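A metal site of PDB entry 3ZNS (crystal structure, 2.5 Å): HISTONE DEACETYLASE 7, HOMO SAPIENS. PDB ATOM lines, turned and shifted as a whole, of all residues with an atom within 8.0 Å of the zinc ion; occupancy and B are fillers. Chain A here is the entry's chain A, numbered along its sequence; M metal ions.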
ATOM      1  N   GLN A  52     -29.863  14.250 -11.810  1.00  0.00           N
ATOM      2  CA  GLN A  52     -28.769  15.047 -12.339  1.00  0.00           C
ATOM      3  C   GLN A  52     -28.685  16.367 -11.580  1.00  0.00           C
ATOM      4  O   GLN A  52     -29.712  16.929 -11.205  1.00  0.00           O
ATOM      5  CB  GLN A  52     -28.943  15.343 -13.835  1.00  0.00           C
ATOM      6  CG  GLN A  52     -29.828  14.356 -14.613  1.00  0.00           C
ATOM      7  CD  GLN A  52     -29.925  14.666 -16.105  1.00  0.00           C
ATOM      8  OE1 GLN A  52     -29.962  13.753 -16.925  1.00  0.00           O
ATOM      9  NE2 GLN A  52     -29.969  15.942 -16.454  1.00  0.00           N
ATOM     10  N   CYS A  53     -27.472  16.868 -11.367  1.00  0.00           N
ATOM     11  CA  CYS A  53     -27.265  18.187 -10.795  1.00  0.00           C
ATOM     12  C   CYS A  53     -27.785  19.266 -11.754  1.00  0.00           C
ATOM     13  O   CYS A  53     -27.753  19.093 -12.974  1.00  0.00           O
ATOM     14  CB  CYS A  53     -25.780  18.410 -10.511  1.00  0.00           C
ATOM     15  SG  CYS A  53     -25.450  19.959  -9.667  1.00  0.00           S
ATOM     16  N   SER A  54     -28.253  20.370 -11.188  1.00  0.00           N
ATOM     17  CA  SER A  54     -28.897  21.426 -11.978  1.00  0.00           C
ATOM     18  C   SER A  54     -27.914  22.210 -12.866  1.00  0.00           C
ATOM     19  O   SER A  54     -28.324  22.816 -13.853  1.00  0.00           O
ATOM     20  CB  SER A  54     -29.660  22.388 -11.065  1.00  0.00           C
ATOM     21  OG  SER A  54     -28.885  22.765  -9.940  1.00  0.00           O
ATOM     22  N   CYS A  55     -26.630  22.179 -12.510  1.00  0.00           N
ATOM     23  CA  CYS A  55     -25.594  22.851 -13.304  1.00  0.00           C
ATOM     24  C   CYS A  55     -25.395  22.213 -14.675  1.00  0.00           C
ATOM     25  O   CYS A  55     -24.848  22.843 -15.573  1.00  0.00           O
ATOM     26  CB  CYS A  55     -24.264  22.860 -12.548  1.00  0.00           C
ATOM     27  SG  CYS A  55     -23.517  21.225 -12.365  1.00  0.00           S
ATOM     28  N   GLY A  56     -25.828  20.957 -14.828  1.00  0.00           N
ATOM     29  CA  GLY A  56     -25.875  20.292 -16.127  1.00  0.00           C
ATOM     30  C   GLY A  56     -24.648  19.476 -16.504  1.00  0.00           C
ATOM     31  O   GLY A  56     -24.738  18.586 -17.354  1.00  0.00           O
ATOM     32  N   ASP A  57     -23.520  19.749 -15.854  1.00  0.00           N
ATOM     33  CA  ASP A  57     -22.230  19.211 -16.273  1.00  0.00           C
ATOM     34  C   ASP A  57     -22.036  17.729 -15.908  1.00  0.00           C
ATOM     35  O   ASP A  57     -21.884  17.376 -14.740  1.00  0.00           O
ATOM     36  CB  ASP A  57     -21.105  20.056 -15.657  1.00  0.00           C
ATOM     37  CG  ASP A  57     -19.822  19.975 -16.448  1.00  0.00           C
ATOM     38  OD1 ASP A  57     -19.529  18.911 -17.027  1.00  0.00           O
ATOM     39  OD2 ASP A  57     -19.112  21.003 -16.507  1.00  0.00           O
ATOM     40  N   ASN A  58     -22.027  16.875 -16.934  1.00  0.00           N
ATOM     41  CA  ASN A  58     -21.815  15.424 -16.750  1.00  0.00           C
ATOM     42  C   ASN A  58     -20.351  15.039 -16.513  1.00  0.00           C
ATOM     43  O   ASN A  58     -20.063  13.891 -16.139  1.00  0.00           O
ATOM     44  CB  ASN A  58     -22.357  14.650 -17.955  1.00  0.00           C
ATOM     45  CG  ASN A  58     -23.868  14.718 -18.060  1.00  0.00           C
ATOM     46  OD1 ASN A  58     -24.590  14.166 -17.222  1.00  0.00           O
ATOM     47  ND2 ASN A  58     -24.359  15.390 -19.094  1.00  0.00           N
ATOM     48  N   ARG A  60     -18.105  17.153 -14.533  1.00  0.00           N
ATOM     49  CA  ARG A  60     -17.942  17.476 -13.111  1.00  0.00           C
ATOM     50  C   ARG A  60     -18.719  16.525 -12.205  1.00  0.00           C
ATOM     51  O   ARG A  60     -18.349  16.331 -11.044  1.00  0.00           O
ATOM     52  CB  ARG A  60     -18.352  18.929 -12.822  1.00  0.00           C
ATOM     53  CG  ARG A  60     -18.241  19.315 -11.341  1.00  0.00           C
ATOM     54  CD  ARG A  60     -18.000  20.802 -11.128  1.00  0.00           C
ATOM     55  NE  ARG A  60     -19.002  21.647 -11.775  1.00  0.00           N
ATOM     56  CZ  ARG A  60     -18.763  22.592 -12.689  1.00  0.00           C
ATOM     57  NH1 ARG A  60     -17.522  22.867 -13.101  1.00  0.00           N
ATOM     58  NH2 ARG A  60     -19.780  23.287 -13.201  1.00  0.00           N
ATOM     59  N   HIS A  61     -19.794  15.922 -12.732  1.00  0.00           N
ATOM     60  CA  HIS A  61     -20.595  14.949 -11.986  1.00  0.00           C
ATOM     61  C   HIS A  61     -20.639  13.620 -12.752  1.00  0.00           C
ATOM     62  O   HIS A  61     -21.594  13.351 -13.478  1.00  0.00           O
ATOM     63  CB  HIS A  61     -21.995  15.502 -11.743  1.00  0.00           C
ATOM     64  CG  HIS A  61     -21.993  16.814 -11.031  1.00  0.00           C
ATOM     65  ND1 HIS A  61     -21.504  16.961  -9.743  1.00  0.00           N
ATOM     66  CD2 HIS A  61     -22.404  18.050 -11.418  1.00  0.00           C
ATOM     67  CE1 HIS A  61     -21.618  18.229  -9.372  1.00  0.00           C
ATOM     68  NE2 HIS A  61     -22.161  18.909 -10.369  1.00  0.00           N
ATOM     69  N   LEU A 136     -22.872  23.867  -3.156  1.00  0.00           N
ATOM     70  CA  LEU A 136     -21.704  23.318  -3.863  1.00  0.00           C
ATOM     71  C   LEU A 136     -20.990  24.430  -4.634  1.00  0.00           C
ATOM     72  O   LEU A 136     -21.592  25.461  -4.904  1.00  0.00           O
ATOM     73  CB  LEU A 136     -22.128  22.212  -4.834  1.00  0.00           C
ATOM     74  CG  LEU A 136     -22.851  20.997  -4.251  1.00  0.00           C
ATOM     75  CD1 LEU A 136     -23.477  20.173  -5.365  1.00  0.00           C
ATOM     76  CD2 LEU A 136     -21.903  20.141  -3.424  1.00  0.00           C
ATOM     77  N   PRO A 137     -19.709  24.208  -4.992  1.00  0.00           N
ATOM     78  CA  PRO A 137     -18.972  25.188  -5.793  1.00  0.00           C
ATOM     79  C   PRO A 137     -19.629  25.520  -7.131  1.00  0.00           C
ATOM     80  O   PRO A 137     -19.535  26.660  -7.599  1.00  0.00           O
ATOM     81  CB  PRO A 137     -17.608  24.510  -6.024  1.00  0.00           C
ATOM     82  CG  PRO A 137     -17.463  23.553  -4.905  1.00  0.00           C
ATOM     83  CD  PRO A 137     -18.847  23.067  -4.604  1.00  0.00           C
ATOM     84  N   CYS A 138     -20.300  24.540  -7.731  1.00  0.00           N
ATOM     85  CA  CYS A 138     -20.956  24.730  -9.027  1.00  0.00           C
ATOM     86  C   CYS A 138     -22.334  25.381  -8.922  1.00  0.00           C
ATOM     87  O   CYS A 138     -22.949  25.701  -9.954  1.00  0.00           O
ATOM     88  CB  CYS A 138     -21.114  23.372  -9.724  1.00  0.00           C
ATOM     89  SG  CYS A 138     -22.290  22.283  -8.901  1.00  0.00           S
ATOM     90  N   GLY A 139     -22.835  25.570  -7.699  1.00  0.00           N
ATOM     91  CA  GLY A 139     -24.121  26.228  -7.483  1.00  0.00           C
ATOM     92  C   GLY A 139     -25.286  25.302  -7.216  1.00  0.00           C
ATOM     93  O   GLY A 139     -26.313  25.740  -6.701  1.00  0.00           O
ATOM     94  N   GLY A 140     -25.156  24.029  -7.587  1.00  0.00           N
ATOM     95  CA  GLY A 140     -26.181  23.033  -7.288  1.00  0.00           C
ATOM     96  C   GLY A 140     -26.162  22.634  -5.829  1.00  0.00           C
ATOM     97  O   GLY A 140     -25.231  22.959  -5.101  1.00  0.00           O
ATOM     98  N   VAL A 141     -27.200  21.927  -5.409  1.00  0.00           N
ATOM     99  CA  VAL A 141     -27.289  21.425  -4.037  1.00  0.00           C
ATOM    100  C   VAL A 141     -26.775  19.979  -4.002  1.00  0.00           C
ATOM    101  O   VAL A 141     -26.850  19.260  -4.997  1.00  0.00           O
ATOM    102  CB  VAL A 141     -28.736  21.518  -3.499  1.00  0.00           C
ATOM    103  CG1 VAL A 141     -28.893  20.737  -2.198  1.00  0.00           C
ATOM    104  CG2 VAL A 141     -29.120  22.973  -3.282  1.00  0.00           C
ATOM    105  N   THR A 145     -19.682  17.018  -1.762  1.00  0.00           N
ATOM    106  CA  THR A 145     -19.177  17.530  -3.032  1.00  0.00           C
ATOM    107  C   THR A 145     -19.443  16.580  -4.198  1.00  0.00           C
ATOM    108  O   THR A 145     -19.636  17.028  -5.331  1.00  0.00           O
ATOM    109  CB  THR A 145     -17.667  17.856  -2.964  1.00  0.00           C
ATOM    110  OG1 THR A 145     -17.363  18.902  -3.897  1.00  0.00           O
ATOM    111  CG2 THR A 145     -16.816  16.629  -3.264  1.00  0.00           C
ATOM    112  N   ILE A 148     -24.595  14.611  -5.284  1.00  0.00           N
ATOM    113  CA  ILE A 148     -25.470  15.733  -5.606  1.00  0.00           C
ATOM    114  C   ILE A 148     -26.918  15.421  -5.250  1.00  0.00           C
ATOM    115  O   ILE A 148     -27.262  14.274  -4.953  1.00  0.00           O
ATOM    116  CB  ILE A 148     -25.365  16.154  -7.113  1.00  0.00           C
ATOM    117  CG1 ILE A 148     -26.015  15.120  -8.042  1.00  0.00           C
ATOM    118  CG2 ILE A 148     -23.905  16.394  -7.498  1.00  0.00           C
ATOM    119  CD1 ILE A 148     -27.483  15.386  -8.317  1.00  0.00           C
HETATM  120 ZN    ZN M   1     -23.242  20.678 -10.379  1.00  0.00          ZN
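Within 4 Å of the zinc ion: Cys 53, Cys 55, His 61 and Cys 138. Along chain A the residues within 4 Å of the zinc ion span positions 53 to 138.
The side-chain sulfur (SG) of Cys 55 lies close to the backbone NH (N) of Asp 57 (3.8 Å). SG of Cys 138 lies close to N of Gly 140 (3.6 Å).
The zinc ion is bound by NE2 of His 61 (2.1 Å), SG of Cys 55 (2.1 Å), SG of Cys 138 (2.4 Å) and SG of Cys 53 (2.4 Å).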
